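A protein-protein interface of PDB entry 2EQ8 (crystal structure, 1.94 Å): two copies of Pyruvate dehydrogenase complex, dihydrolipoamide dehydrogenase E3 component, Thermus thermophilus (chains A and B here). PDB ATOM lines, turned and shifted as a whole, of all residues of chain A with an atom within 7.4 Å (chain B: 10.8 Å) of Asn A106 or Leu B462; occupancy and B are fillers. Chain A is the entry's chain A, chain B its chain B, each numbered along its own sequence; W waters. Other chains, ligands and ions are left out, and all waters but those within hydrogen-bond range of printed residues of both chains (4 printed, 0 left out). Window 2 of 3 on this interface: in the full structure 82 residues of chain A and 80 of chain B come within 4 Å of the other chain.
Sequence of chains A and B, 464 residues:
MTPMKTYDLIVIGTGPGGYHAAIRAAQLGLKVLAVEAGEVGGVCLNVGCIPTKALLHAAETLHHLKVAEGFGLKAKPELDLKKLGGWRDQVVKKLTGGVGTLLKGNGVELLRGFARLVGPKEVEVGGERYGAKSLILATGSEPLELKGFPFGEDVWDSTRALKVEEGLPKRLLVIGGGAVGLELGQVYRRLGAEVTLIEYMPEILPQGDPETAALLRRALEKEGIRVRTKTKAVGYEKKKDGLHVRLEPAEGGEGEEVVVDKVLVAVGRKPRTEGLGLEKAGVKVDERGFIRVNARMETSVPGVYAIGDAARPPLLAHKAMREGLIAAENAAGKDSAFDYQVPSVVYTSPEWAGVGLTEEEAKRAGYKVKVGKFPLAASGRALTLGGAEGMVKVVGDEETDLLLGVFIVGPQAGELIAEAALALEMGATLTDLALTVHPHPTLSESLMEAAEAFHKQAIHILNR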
ATOM      1  N   TYR A  19     -36.505 -15.644 -13.347  1.00  0.00           N
ATOM      2  CA  TYR A  19     -35.089 -15.843 -13.604  1.00  0.00           C
ATOM      3  C   TYR A  19     -34.829 -16.471 -14.969  1.00  0.00           C
ATOM      4  O   TYR A  19     -33.762 -16.282 -15.547  1.00  0.00           O
ATOM      5  CB  TYR A  19     -34.406 -16.593 -12.438  1.00  0.00           C
ATOM      6  CG  TYR A  19     -34.514 -18.103 -12.361  1.00  0.00           C
ATOM      7  CD1 TYR A  19     -33.822 -18.922 -13.251  1.00  0.00           C
ATOM      8  CD2 TYR A  19     -35.231 -18.714 -11.327  1.00  0.00           C
ATOM      9  CE1 TYR A  19     -33.834 -20.309 -13.113  1.00  0.00           C
ATOM     10  CE2 TYR A  19     -35.253 -20.099 -11.181  1.00  0.00           C
ATOM     11  CZ  TYR A  19     -34.551 -20.890 -12.077  1.00  0.00           C
ATOM     12  OH  TYR A  19     -34.560 -22.258 -11.938  1.00  0.00           O
ATOM     13  N   ALA A  22     -35.161 -13.397 -17.292  1.00  0.00           N
ATOM     14  CA  ALA A  22     -33.996 -12.533 -17.166  1.00  0.00           C
ATOM     15  C   ALA A  22     -32.793 -13.122 -17.892  1.00  0.00           C
ATOM     16  O   ALA A  22     -32.120 -12.431 -18.662  1.00  0.00           O
ATOM     17  CB  ALA A  22     -33.660 -12.316 -15.695  1.00  0.00           C
ATOM     18  N   ILE A  23     -32.526 -14.402 -17.643  1.00  0.00           N
ATOM     19  CA  ILE A  23     -31.391 -15.076 -18.260  1.00  0.00           C
ATOM     20  C   ILE A  23     -31.487 -15.188 -19.776  1.00  0.00           C
ATOM     21  O   ILE A  23     -30.517 -14.910 -20.478  1.00  0.00           O
ATOM     22  CB  ILE A  23     -31.187 -16.481 -17.631  1.00  0.00           C
ATOM     23  CG1 ILE A  23     -30.768 -16.314 -16.167  1.00  0.00           C
ATOM     24  CG2 ILE A  23     -30.135 -17.271 -18.404  1.00  0.00           C
ATOM     25  CD1 ILE A  23     -30.682 -17.610 -15.382  1.00  0.00           C
ATOM     26  N   ARG A  24     -32.650 -15.581 -20.290  1.00  0.00           N
ATOM     27  CA  ARG A  24     -32.813 -15.712 -21.733  1.00  0.00           C
ATOM     28  C   ARG A  24     -32.677 -14.339 -22.404  1.00  0.00           C
ATOM     29  O   ARG A  24     -32.071 -14.216 -23.465  1.00  0.00           O
ATOM     30  CB  ARG A  24     -34.172 -16.361 -22.045  1.00  0.00           C
ATOM     31  CG  ARG A  24     -34.470 -16.587 -23.522  1.00  0.00           C
ATOM     32  CD  ARG A  24     -33.304 -17.207 -24.299  1.00  0.00           C
ATOM     33  NE  ARG A  24     -32.923 -18.563 -23.895  1.00  0.00           N
ATOM     34  CZ  ARG A  24     -33.610 -19.671 -24.168  1.00  0.00           C
ATOM     35  NH1 ARG A  24     -34.747 -19.618 -24.849  1.00  0.00           N
ATOM     36  NH2 ARG A  24     -33.136 -20.852 -23.786  1.00  0.00           N
ATOM     37  N   ALA A  25     -33.222 -13.307 -21.768  1.00  0.00           N
ATOM     38  CA  ALA A  25     -33.139 -11.953 -22.298  1.00  0.00           C
ATOM     39  C   ALA A  25     -31.672 -11.537 -22.371  1.00  0.00           C
ATOM     40  O   ALA A  25     -31.227 -10.945 -23.357  1.00  0.00           O
ATOM     41  CB  ALA A  25     -33.917 -10.993 -21.405  1.00  0.00           C
ATOM     42  N   ALA A  26     -30.918 -11.855 -21.325  1.00  0.00           N
ATOM     43  CA  ALA A  26     -29.502 -11.515 -21.290  1.00  0.00           C
ATOM     44  C   ALA A  26     -28.746 -12.256 -22.389  1.00  0.00           C
ATOM     45  O   ALA A  26     -27.821 -11.710 -22.991  1.00  0.00           O
ATOM     46  CB  ALA A  26     -28.913 -11.852 -19.931  1.00  0.00           C
ATOM     47  N   GLN A  27     -29.145 -13.498 -22.654  1.00  0.00           N
ATOM     48  CA  GLN A  27     -28.502 -14.296 -23.691  1.00  0.00           C
ATOM     49  C   GLN A  27     -28.751 -13.683 -25.064  1.00  0.00           C
ATOM     50  O   GLN A  27     -27.919 -13.809 -25.963  1.00  0.00           O
ATOM     51  CB  GLN A  27     -29.033 -15.732 -23.678  1.00  0.00           C
ATOM     52  CG  GLN A  27     -28.830 -16.465 -22.357  1.00  0.00           C
ATOM     53  CD  GLN A  27     -29.485 -17.833 -22.347  1.00  0.00           C
ATOM     54  OE1 GLN A  27     -30.522 -18.035 -22.976  1.00  0.00           O
ATOM     55  NE2 GLN A  27     -28.896 -18.772 -21.619  1.00  0.00           N
ATOM     56  N   LEU A  30     -29.949  -8.321 -24.206  1.00  0.00           N
ATOM     57  CA  LEU A  30     -30.654  -7.229 -23.537  1.00  0.00           C
ATOM     58  C   LEU A  30     -30.025  -6.910 -22.186  1.00  0.00           C
ATOM     59  O   LEU A  30     -29.479  -7.797 -21.530  1.00  0.00           O
ATOM     60  CB  LEU A  30     -32.128  -7.588 -23.329  1.00  0.00           C
ATOM     61  CG  LEU A  30     -32.965  -7.917 -24.567  1.00  0.00           C
ATOM     62  CD1 LEU A  30     -34.394  -8.214 -24.136  1.00  0.00           C
ATOM     63  CD2 LEU A  30     -32.941  -6.756 -25.549  1.00  0.00           C
ATOM     64  N   VAL A  32     -30.586  -6.336 -18.584  1.00  0.00           N
ATOM     65  CA  VAL A  32     -31.671  -6.670 -17.672  1.00  0.00           C
ATOM     66  C   VAL A  32     -31.521  -6.260 -16.219  1.00  0.00           C
ATOM     67  O   VAL A  32     -30.437  -6.301 -15.650  1.00  0.00           O
ATOM     68  CB  VAL A  32     -31.923  -8.198 -17.690  1.00  0.00           C
ATOM     69  CG1 VAL A  32     -33.136  -8.543 -16.841  1.00  0.00           C
ATOM     70  CG2 VAL A  32     -32.105  -8.679 -19.126  1.00  0.00           C
ATOM     71  N   VAL A  99     -29.067 -19.625  -8.392  1.00  0.00           N
ATOM     72  CA  VAL A  99     -29.811 -18.731  -9.274  1.00  0.00           C
ATOM     73  C   VAL A  99     -29.149 -17.357  -9.263  1.00  0.00           C
ATOM     74  O   VAL A  99     -29.005 -16.719 -10.308  1.00  0.00           O
ATOM     75  CB  VAL A  99     -31.290 -18.590  -8.834  1.00  0.00           C
ATOM     76  CG1 VAL A  99     -32.000 -17.557  -9.707  1.00  0.00           C
ATOM     77  CG2 VAL A  99     -31.996 -19.934  -8.950  1.00  0.00           C
ATOM     78  N   GLY A 100     -28.747 -16.904  -8.080  1.00  0.00           N
ATOM     79  CA  GLY A 100     -28.090 -15.612  -7.983  1.00  0.00           C
ATOM     80  C   GLY A 100     -26.788 -15.617  -8.766  1.00  0.00           C
ATOM     81  O   GLY A 100     -26.425 -14.627  -9.402  1.00  0.00           O
ATOM     82  N   THR A 101     -26.085 -16.742  -8.727  1.00  0.00           N
ATOM     83  CA  THR A 101     -24.819 -16.874  -9.438  1.00  0.00           C
ATOM     84  C   THR A 101     -25.038 -16.865 -10.944  1.00  0.00           C
ATOM     85  O   THR A 101     -24.246 -16.293 -11.688  1.00  0.00           O
ATOM     86  CB  THR A 101     -24.086 -18.165  -9.031  1.00  0.00           C
ATOM     87  OG1 THR A 101     -23.803 -18.121  -7.628  1.00  0.00           O
ATOM     88  CG2 THR A 101     -22.779 -18.309  -9.793  1.00  0.00           C
ATOM     89  N   LEU A 102     -26.117 -17.497 -11.392  1.00  0.00           N
ATOM     90  CA  LEU A 102     -26.432 -17.528 -12.811  1.00  0.00           C
ATOM     91  C   LEU A 102     -26.832 -16.139 -13.297  1.00  0.00           C
ATOM     92  O   LEU A 102     -26.415 -15.707 -14.369  1.00  0.00           O
ATOM     93  CB  LEU A 102     -27.556 -18.534 -13.084  1.00  0.00           C
ATOM     94  CG  LEU A 102     -27.090 -19.992 -13.033  1.00  0.00           C
ATOM     95  CD1 LEU A 102     -28.287 -20.923 -12.870  1.00  0.00           C
ATOM     96  CD2 LEU A 102     -26.323 -20.310 -14.305  1.00  0.00           C
ATOM     97  N   LEU A 103     -27.638 -15.436 -12.509  1.00  0.00           N
ATOM     98  CA  LEU A 103     -28.059 -14.094 -12.892  1.00  0.00           C
ATOM     99  C   LEU A 103     -26.834 -13.206 -13.071  1.00  0.00           C
ATOM    100  O   LEU A 103     -26.683 -12.534 -14.092  1.00  0.00           O
ATOM    101  CB  LEU A 103     -28.979 -13.499 -11.825  1.00  0.00           C
ATOM    102  CG  LEU A 103     -30.384 -14.103 -11.746  1.00  0.00           C
ATOM    103  CD1 LEU A 103     -31.167 -13.413 -10.637  1.00  0.00           C
ATOM    104  CD2 LEU A 103     -31.096 -13.941 -13.089  1.00  0.00           C
ATOM    105  N   LYS A 104     -25.952 -13.213 -12.079  1.00  0.00           N
ATOM    106  CA  LYS A 104     -24.752 -12.396 -12.157  1.00  0.00           C
ATOM    107  C   LYS A 104     -23.874 -12.828 -13.328  1.00  0.00           C
ATOM    108  O   LYS A 104     -23.332 -11.991 -14.052  1.00  0.00           O
ATOM    109  CB  LYS A 104     -23.947 -12.485 -10.860  1.00  0.00           C
ATOM    110  CG  LYS A 104     -22.990 -11.315 -10.706  1.00  0.00           C
ATOM    111  CD  LYS A 104     -21.831 -11.615  -9.787  1.00  0.00           C
ATOM    112  CE  LYS A 104     -20.876 -10.432  -9.763  1.00  0.00           C
ATOM    113  NZ  LYS A 104     -20.529  -9.995 -11.149  1.00  0.00           N
ATOM    114  N   GLY A 105     -23.737 -14.140 -13.506  1.00  0.00           N
ATOM    115  CA  GLY A 105     -22.923 -14.665 -14.588  1.00  0.00           C
ATOM    116  C   GLY A 105     -23.426 -14.265 -15.961  1.00  0.00           C
ATOM    117  O   GLY A 105     -22.679 -14.302 -16.943  1.00  0.00           O
ATOM    118  N   ASN A 106     -24.700 -13.887 -16.033  1.00  0.00           N
ATOM    119  CA  ASN A 106     -25.311 -13.469 -17.291  1.00  0.00           C
ATOM    120  C   ASN A 106     -25.361 -11.950 -17.434  1.00  0.00           C
ATOM    121  O   ASN A 106     -25.917 -11.427 -18.398  1.00  0.00           O
ATOM    122  CB  ASN A 106     -26.726 -14.041 -17.397  1.00  0.00           C
ATOM    123  CG  ASN A 106     -26.736 -15.464 -17.892  1.00  0.00           C
ATOM    124  OD1 ASN A 106     -26.626 -15.714 -19.095  1.00  0.00           O
ATOM    125  ND2 ASN A 106     -26.848 -16.411 -16.966  1.00  0.00           N
ATOM    126  N   GLY A 107     -24.783 -11.248 -16.468  1.00  0.00           N
ATOM    127  CA  GLY A 107     -24.775  -9.799 -16.518  1.00  0.00           C
ATOM    128  C   GLY A 107     -26.073  -9.153 -16.075  1.00  0.00           C
ATOM    129  O   GLY A 107     -26.308  -7.986 -16.363  1.00  0.00           O
ATOM    130  N   VAL A 108     -26.918  -9.905 -15.376  1.00  0.00           N
ATOM    131  CA  VAL A 108     -28.191  -9.368 -14.903  1.00  0.00           C
ATOM    132  C   VAL A 108     -28.012  -8.622 -13.583  1.00  0.00           C
ATOM    133  O   VAL A 108     -27.349  -9.109 -12.670  1.00  0.00           O
ATOM    134  CB  VAL A 108     -29.242 -10.491 -14.699  1.00  0.00           C
ATOM    135  CG1 VAL A 108     -30.508  -9.921 -14.084  1.00  0.00           C
ATOM    136  CG2 VAL A 108     -29.564 -11.148 -16.032  1.00  0.00           C
ATOM    137  N   GLU A 109     -28.594  -7.432 -13.498  1.00  0.00           N
ATOM    138  CA  GLU A 109     -28.520  -6.636 -12.279  1.00  0.00           C
ATOM    139  C   GLU A 109     -29.676  -7.053 -11.368  1.00  0.00           C
ATOM    140  O   GLU A 109     -30.830  -7.072 -11.793  1.00  0.00           O
ATOM    141  CB  GLU A 109     -28.631  -5.145 -12.614  1.00  0.00           C
ATOM    142  CG  GLU A 109     -27.471  -4.299 -12.116  1.00  0.00           C
ATOM    143  CD  GLU A 109     -27.811  -3.499 -10.874  1.00  0.00           C
ATOM    144  OE1 GLU A 109     -28.768  -2.696 -10.925  1.00  0.00           O
ATOM    145  OE2 GLU A 109     -27.118  -3.666  -9.848  1.00  0.00           O
ATOM    146  N   GLY B 372     -24.247 -31.215 -27.196  1.00  0.00           N
ATOM    147  CA  GLY B 372     -24.804 -30.406 -26.133  1.00  0.00           C
ATOM    148  C   GLY B 372     -24.619 -31.230 -24.873  1.00  0.00           C
ATOM    149  O   GLY B 372     -24.888 -32.432 -24.890  1.00  0.00           O
ATOM    150  N   LYS B 373     -24.160 -30.605 -23.793  1.00  0.00           N
ATOM    151  CA  LYS B 373     -23.928 -31.324 -22.538  1.00  0.00           C
ATOM    152  C   LYS B 373     -24.542 -30.605 -21.342  1.00  0.00           C
ATOM    153  O   LYS B 373     -24.516 -29.382 -21.265  1.00  0.00           O
ATOM    154  CB  LYS B 373     -22.427 -31.484 -22.299  1.00  0.00           C
ATOM    155  CG  LYS B 373     -21.670 -32.121 -23.456  1.00  0.00           C
ATOM    156  CD  LYS B 373     -20.177 -32.173 -23.164  1.00  0.00           C
ATOM    157  CE  LYS B 373     -19.392 -32.698 -24.351  1.00  0.00           C
ATOM    158  NZ  LYS B 373     -17.922 -32.706 -24.074  1.00  0.00           N
ATOM    159  N   PHE B 374     -25.092 -31.371 -20.405  1.00  0.00           N
ATOM    160  CA  PHE B 374     -25.688 -30.790 -19.215  1.00  0.00           C
ATOM    161  C   PHE B 374     -25.344 -31.664 -18.011  1.00  0.00           C
ATOM    162  O   PHE B 374     -25.703 -32.842 -17.974  1.00  0.00           O
ATOM    163  CB  PHE B 374     -27.208 -30.690 -19.359  1.00  0.00           C
ATOM    164  CG  PHE B 374     -27.860 -29.909 -18.253  1.00  0.00           C
ATOM    165  CD1 PHE B 374     -27.831 -28.520 -18.255  1.00  0.00           C
ATOM    166  CD2 PHE B 374     -28.461 -30.565 -17.182  1.00  0.00           C
ATOM    167  CE1 PHE B 374     -28.389 -27.789 -17.202  1.00  0.00           C
ATOM    168  CE2 PHE B 374     -29.023 -29.842 -16.120  1.00  0.00           C
ATOM    169  CZ  PHE B 374     -28.986 -28.453 -16.133  1.00  0.00           C
ATOM    170  N   PRO B 375     -24.639 -31.094 -17.016  1.00  0.00           N
ATOM    171  CA  PRO B 375     -24.226 -31.800 -15.801  1.00  0.00           C
ATOM    172  C   PRO B 375     -25.337 -31.857 -14.762  1.00  0.00           C
ATOM    173  O   PRO B 375     -26.114 -30.914 -14.628  1.00  0.00           O
ATOM    174  CB  PRO B 375     -23.034 -30.978 -15.325  1.00  0.00           C
ATOM    175  CG  PRO B 375     -23.488 -29.590 -15.627  1.00  0.00           C
ATOM    176  CD  PRO B 375     -24.095 -29.722 -17.023  1.00  0.00           C
ATOM    177  N   ALA B 377     -25.004 -31.697 -11.658  1.00  0.00           N
ATOM    178  CA  ALA B 377     -24.703 -30.785 -10.559  1.00  0.00           C
ATOM    179  C   ALA B 377     -25.623 -29.568 -10.611  1.00  0.00           C
ATOM    180  O   ALA B 377     -25.881 -28.928  -9.589  1.00  0.00           O
ATOM    181  CB  ALA B 377     -23.243 -30.341 -10.637  1.00  0.00           C
ATOM    182  N   ALA B 378     -26.125 -29.254 -11.804  1.00  0.00           N
ATOM    183  CA  ALA B 378     -27.009 -28.106 -11.985  1.00  0.00           C
ATOM    184  C   ALA B 378     -28.483 -28.497 -11.944  1.00  0.00           C
ATOM    185  O   ALA B 378     -29.344 -27.713 -12.348  1.00  0.00           O
ATOM    186  CB  ALA B 378     -26.694 -27.410 -13.315  1.00  0.00           C
ATOM    187  N   GLU B 449     -32.339 -29.525 -21.238  1.00  0.00           N
ATOM    188  CA  GLU B 449     -31.290 -28.519 -21.095  1.00  0.00           C
ATOM    189  C   GLU B 449     -30.033 -28.850 -21.900  1.00  0.00           C
ATOM    190  O   GLU B 449     -29.302 -27.945 -22.318  1.00  0.00           O
ATOM    191  CB  GLU B 449     -30.956 -28.309 -19.612  1.00  0.00           C
ATOM    192  CG  GLU B 449     -32.150 -27.790 -18.796  1.00  0.00           C
ATOM    193  CD  GLU B 449     -31.736 -26.955 -17.599  1.00  0.00           C
ATOM    194  OE1 GLU B 449     -31.095 -25.895 -17.802  1.00  0.00           O
ATOM    195  OE2 GLU B 449     -32.050 -27.355 -16.456  1.00  0.00           O
ATOM    196  N   GLU B 452     -30.768 -27.449 -24.997  1.00  0.00           N
ATOM    197  CA  GLU B 452     -30.627 -25.987 -24.929  1.00  0.00           C
ATOM    198  C   GLU B 452     -29.137 -25.658 -25.061  1.00  0.00           C
ATOM    199  O   GLU B 452     -28.750 -24.734 -25.780  1.00  0.00           O
ATOM    200  CB  GLU B 452     -31.116 -25.435 -23.578  1.00  0.00           C
ATOM    201  CG  GLU B 452     -32.543 -25.784 -23.171  1.00  0.00           C
ATOM    202  CD  GLU B 452     -32.839 -25.451 -21.695  1.00  0.00           C
ATOM    203  OE1 GLU B 452     -34.012 -25.588 -21.270  1.00  0.00           O
ATOM    204  OE2 GLU B 452     -31.903 -25.057 -20.954  1.00  0.00           O
ATOM    205  N   ALA B 453     -28.310 -26.419 -24.347  1.00  0.00           N
ATOM    206  CA  ALA B 453     -26.861 -26.230 -24.367  1.00  0.00           C
ATOM    207  C   ALA B 453     -26.273 -26.418 -25.767  1.00  0.00           C
ATOM    208  O   ALA B 453     -25.298 -25.761 -26.128  1.00  0.00           O
ATOM    209  CB  ALA B 453     -26.195 -27.188 -23.390  1.00  0.00           C
ATOM    210  N   PHE B 454     -26.860 -27.326 -26.541  1.00  0.00           N
ATOM    211  CA  PHE B 454     -26.425 -27.595 -27.910  1.00  0.00           C
ATOM    212  C   PHE B 454     -26.514 -26.296 -28.714  1.00  0.00           C
ATOM    213  O   PHE B 454     -25.711 -26.053 -29.620  1.00  0.00           O
ATOM    214  CB  PHE B 454     -27.326 -28.678 -28.522  1.00  0.00           C
ATOM    215  CG  PHE B 454     -27.068 -28.964 -29.981  1.00  0.00           C
ATOM    216  CD1 PHE B 454     -27.494 -28.082 -30.970  1.00  0.00           C
ATOM    217  CD2 PHE B 454     -26.462 -30.156 -30.369  1.00  0.00           C
ATOM    218  CE1 PHE B 454     -27.328 -28.390 -32.325  1.00  0.00           C
ATOM    219  CE2 PHE B 454     -26.292 -30.471 -31.718  1.00  0.00           C
ATOM    220  CZ  PHE B 454     -26.727 -29.588 -32.694  1.00  0.00           C
ATOM    221  N   HIS B 455     -27.492 -25.462 -28.371  1.00  0.00           N
ATOM    222  CA  HIS B 455     -27.683 -24.182 -29.046  1.00  0.00           C
ATOM    223  C   HIS B 455     -27.151 -23.020 -28.209  1.00  0.00           C
ATOM    224  O   HIS B 455     -27.542 -21.868 -28.402  1.00  0.00           O
ATOM    225  CB  HIS B 455     -29.163 -23.972 -29.371  1.00  0.00           C
ATOM    226  CG  HIS B 455     -29.674 -24.885 -30.441  1.00  0.00           C
ATOM    227  ND1 HIS B 455     -30.809 -25.652 -30.290  1.00  0.00           N
ATOM    228  CD2 HIS B 455     -29.188 -25.171 -31.673  1.00  0.00           C
ATOM    229  CE1 HIS B 455     -30.998 -26.374 -31.380  1.00  0.00           C
ATOM    230  NE2 HIS B 455     -30.029 -26.101 -32.233  1.00  0.00           N
ATOM    231  N   LYS B 456     -26.268 -23.343 -27.271  1.00  0.00           N
ATOM    232  CA  LYS B 456     -25.633 -22.351 -26.407  1.00  0.00           C
ATOM    233  C   LYS B 456     -26.583 -21.470 -25.602  1.00  0.00           C
ATOM    234  O   LYS B 456     -26.253 -20.321 -25.305  1.00  0.00           O
ATOM    235  CB  LYS B 456     -24.710 -21.448 -27.240  1.00  0.00           C
ATOM    236  CG  LYS B 456     -23.652 -22.193 -28.044  1.00  0.00           C
ATOM    237  CD  LYS B 456     -22.698 -22.946 -27.134  1.00  0.00           C
ATOM    238  CE  LYS B 456     -21.636 -23.693 -27.926  1.00  0.00           C
ATOM    239  NZ  LYS B 456     -20.772 -24.520 -27.030  1.00  0.00           N
ATOM    240  N   GLN B 457     -27.756 -21.987 -25.248  1.00  0.00           N
ATOM    241  CA  GLN B 457     -28.688 -21.187 -24.464  1.00  0.00           C
ATOM    242  C   GLN B 457     -29.293 -21.895 -23.253  1.00  0.00           C
ATOM    243  O   GLN B 457     -30.417 -21.589 -22.861  1.00  0.00           O
ATOM    244  CB  GLN B 457     -29.810 -20.623 -25.351  1.00  0.00           C
ATOM    245  CG  GLN B 457     -30.533 -21.626 -26.231  1.00  0.00           C
ATOM    246  CD  GLN B 457     -31.665 -20.982 -27.008  1.00  0.00           C
ATOM    247  OE1 GLN B 457     -31.623 -19.788 -27.311  1.00  0.00           O
ATOM    248  NE2 GLN B 457     -32.677 -21.770 -27.344  1.00  0.00           N
ATOM    249  N   ALA B 458     -28.550 -22.829 -22.661  1.00  0.00           N
ATOM    250  CA  ALA B 458     -29.036 -23.532 -21.472  1.00  0.00           C
ATOM    251  C   ALA B 458     -29.194 -22.468 -20.393  1.00  0.00           C
ATOM    252  O   ALA B 458     -28.422 -21.509 -20.341  1.00  0.00           O
ATOM    253  CB  ALA B 458     -28.036 -24.595 -21.031  1.00  0.00           C
ATOM    254  N   ILE B 459     -30.190 -22.639 -19.534  1.00  0.00           N
ATOM    255  CA  ILE B 459     -30.473 -21.668 -18.483  1.00  0.00           C
ATOM    256  C   ILE B 459     -29.719 -21.890 -17.179  1.00  0.00           C
ATOM    257  O   ILE B 459     -29.184 -20.942 -16.598  1.00  0.00           O
ATOM    258  CB  ILE B 459     -31.987 -21.644 -18.156  1.00  0.00           C
ATOM    259  CG1 ILE B 459     -32.799 -21.383 -19.429  1.00  0.00           C
ATOM    260  CG2 ILE B 459     -32.280 -20.589 -17.098  1.00  0.00           C
ATOM    261  CD1 ILE B 459     -32.552 -20.023 -20.066  1.00  0.00           C
ATOM    262  N   HIS B 460     -29.672 -23.138 -16.719  1.00  0.00           N
ATOM    263  CA  HIS B 460     -29.022 -23.443 -15.451  1.00  0.00           C
ATOM    264  C   HIS B 460     -27.512 -23.627 -15.435  1.00  0.00           C
ATOM    265  O   HIS B 460     -26.944 -24.017 -14.419  1.00  0.00           O
ATOM    266  CB  HIS B 460     -29.704 -24.645 -14.807  1.00  0.00           C
ATOM    267  CG  HIS B 460     -31.114 -24.374 -14.394  1.00  0.00           C
ATOM    268  ND1 HIS B 460     -32.199 -24.944 -15.023  1.00  0.00           N
ATOM    269  CD2 HIS B 460     -31.618 -23.569 -13.428  1.00  0.00           C
ATOM    270  CE1 HIS B 460     -33.311 -24.505 -14.462  1.00  0.00           C
ATOM    271  NE2 HIS B 460     -32.986 -23.668 -13.492  1.00  0.00           N
ATOM    272  N   ILE B 461     -26.858 -23.366 -16.559  1.00  0.00           N
ATOM    273  CA  ILE B 461     -25.403 -23.448 -16.601  1.00  0.00           C
ATOM    274  C   ILE B 461     -24.931 -22.316 -17.487  1.00  0.00           C
ATOM    275  O   ILE B 461     -25.667 -21.865 -18.363  1.00  0.00           O
ATOM    276  CB  ILE B 461     -24.877 -24.785 -17.184  1.00  0.00           C
ATOM    277  CG1 ILE B 461     -25.382 -24.973 -18.617  1.00  0.00           C
ATOM    278  CG2 ILE B 461     -25.277 -25.946 -16.278  1.00  0.00           C
ATOM    279  CD1 ILE B 461     -24.860 -26.235 -19.291  1.00  0.00           C
ATOM    280  N   LEU B 462     -23.723 -21.832 -17.239  1.00  0.00           N
ATOM    281  CA  LEU B 462     -23.177 -20.765 -18.057  1.00  0.00           C
ATOM    282  C   LEU B 462     -22.743 -21.396 -19.369  1.00  0.00           C
ATOM    283  O   LEU B 462     -22.092 -22.439 -19.376  1.00  0.00           O
ATOM    284  CB  LEU B 462     -21.984 -20.111 -17.360  1.00  0.00           C
ATOM    285  CG  LEU B 462     -22.328 -19.351 -16.078  1.00  0.00           C
ATOM    286  CD1 LEU B 462     -21.078 -18.652 -15.556  1.00  0.00           C
ATOM    287  CD2 LEU B 462     -23.430 -18.330 -16.362  1.00  0.00           C
ATOM    288  N   ASN B 463     -23.116 -20.768 -20.478  1.00  0.00           N
ATOM    289  CA  ASN B 463     -22.778 -21.284 -21.798  1.00  0.00           C
ATOM    290  C   ASN B 463     -21.436 -20.735 -22.275  1.00  0.00           C
ATOM    291  O   ASN B 463     -20.545 -21.549 -22.601  1.00  0.00           O
ATOM    292  CB  ASN B 463     -23.884 -20.918 -22.794  1.00  0.00           C
ATOM    293  CG  ASN B 463     -25.235 -21.524 -22.419  1.00  0.00           C
ATOM    294  OD1 ASN B 463     -25.552 -22.656 -22.795  1.00  0.00           O
ATOM    295  ND2 ASN B 463     -26.028 -20.773 -21.662  1.00  0.00           N
HETATM  296  O   HOH W   1     -27.213 -19.415 -17.649  1.00  0.00           O
HETATM  297  O   HOH W   2     -33.025 -24.041 -10.335  1.00  0.00           O
HETATM  298  O   HOH W   3     -26.837 -18.111 -20.308  1.00  0.00           O
HETATM  299  O   HOH W   4     -30.671 -17.193 -26.288  1.00  0.00           O
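Ile A23 touches just one residue of chain B: Ile B459.
No residue of chain B comes within 4 Å of Ala A26.
Printed residues of chain B within 4 Å of Gln A27: Gln B457 (3.4 Å), Ala B458 (3.1 Å) and Asn B463 (3.5 Å).
Gly A107 touches none of the printed residues of chain B.
No residue of chain B comes within 4 Å of Val A108.
Glu B449 touches none of the printed residues of chain A.
Of the printed residues of chain A, Gln B457 touches Arg A24 (3.0 Å) and Gln A27 (3.4 Å).
Of the printed residues of chain A, Ala B458 touches Gln A27 (3.1 Å).
Printed residues of chain A within 4 Å of His B460: Tyr A19 (2.6 Å) and Leu A102 (3.7 Å).
Leu B462 touches one residue of chain A.
Of the 20 printed residues of chain A, 6 touch a printed residue of chain B.
Hydrophobic or aromatic side chains of chain A that line the printed part of chain B: Tyr A19, Ile A23 and Leu A102.
Of the 19 printed residues of chain B, 7 touch a printed residue of chain A.
Printed residues of chain B that touch a printed residue of chain A: Gln B457, Ala B458, Ile B459, His B460, Ile B461, Leu B462 and Asn B463.
Hydrophobic or aromatic side chains of chain B within 4 Å of the printed part of chain A: Ile B459, His B460 and Leu B462.
Among the printed residues, 11 pairs touch across the chains.
Water W3 lies within hydrogen-bond range of NE2 of Gln A27 (2.5 Å), OD1 of Asn A106 (2.7 Å) and ND2 of Asn B463 (3.1 Å).
Water W1 lies within hydrogen-bond range of O of Ile B459, O of Ile B461 and ND2 of Asn A106.
Water W2 bridges OH of Tyr A19 (2.8 Å) and NE2 of His B460 (3.2 Å).
Water W4 bridges the side-chain amide oxygen (OE1) of Gln B457 (2.9 Å) and the side-chain amide oxygen (OE1) of Gln A27 (3.4 Å).
OH of Tyr A19 is in hydrogen-bond range of NE2 of His B460 (2.6 Å).
The guanidinium group (NH2) of Arg A24 sits at hydrogen-bond distance from the backbone carbonyl oxygen (O) of Gln B457 (3.0 Å).
NE2 of Gln A27 is in hydrogen-bond range of O of Gln B457 (3.4 Å).
O of Ala B458 lies within hydrogen-bond range of NE2 of Gln A27.
NE2 of Gln A27 lies close to ND2 of Asn B463 (3.5 Å).
Ile A23 touches Ile B459 (CD1 to CG2, 3.8 Å).
Arg A24 touches Ile B459 (NH2 to CD1, 3.9 Å).
Ile B459 touches Leu A102 (O to CD2, 3.7 Å).
Leu A102 touches His B460 (CD1 to CA, 3.7 Å).
CD2 of Leu A102 touches N of Ile B461, at 3.8 Å.
Leu B462 touches Asn A106 (CD2 to ND2, 3.97 Å).
No position is printed for both chains.
O of Leu A102 sits at hydrogen-bond distance from ND2 of Asn A106 (2.7 Å).
The backbone carbonyl oxygen (O) of Glu B452 is in hydrogen-bond range of the backbone NH (N) of Gln B457, 3.0 Å away.
The backbone NH of Ile B459 is in hydrogen-bond range of the side-chain carboxylate of Glu B452, 3.3 Å away.
OD1 of Asn B463 lies within hydrogen-bond range of N of Gln B457 (3.4 Å).
O of Ala B458 is in hydrogen-bond range of ND2 of Asn B463 (2.8 Å).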
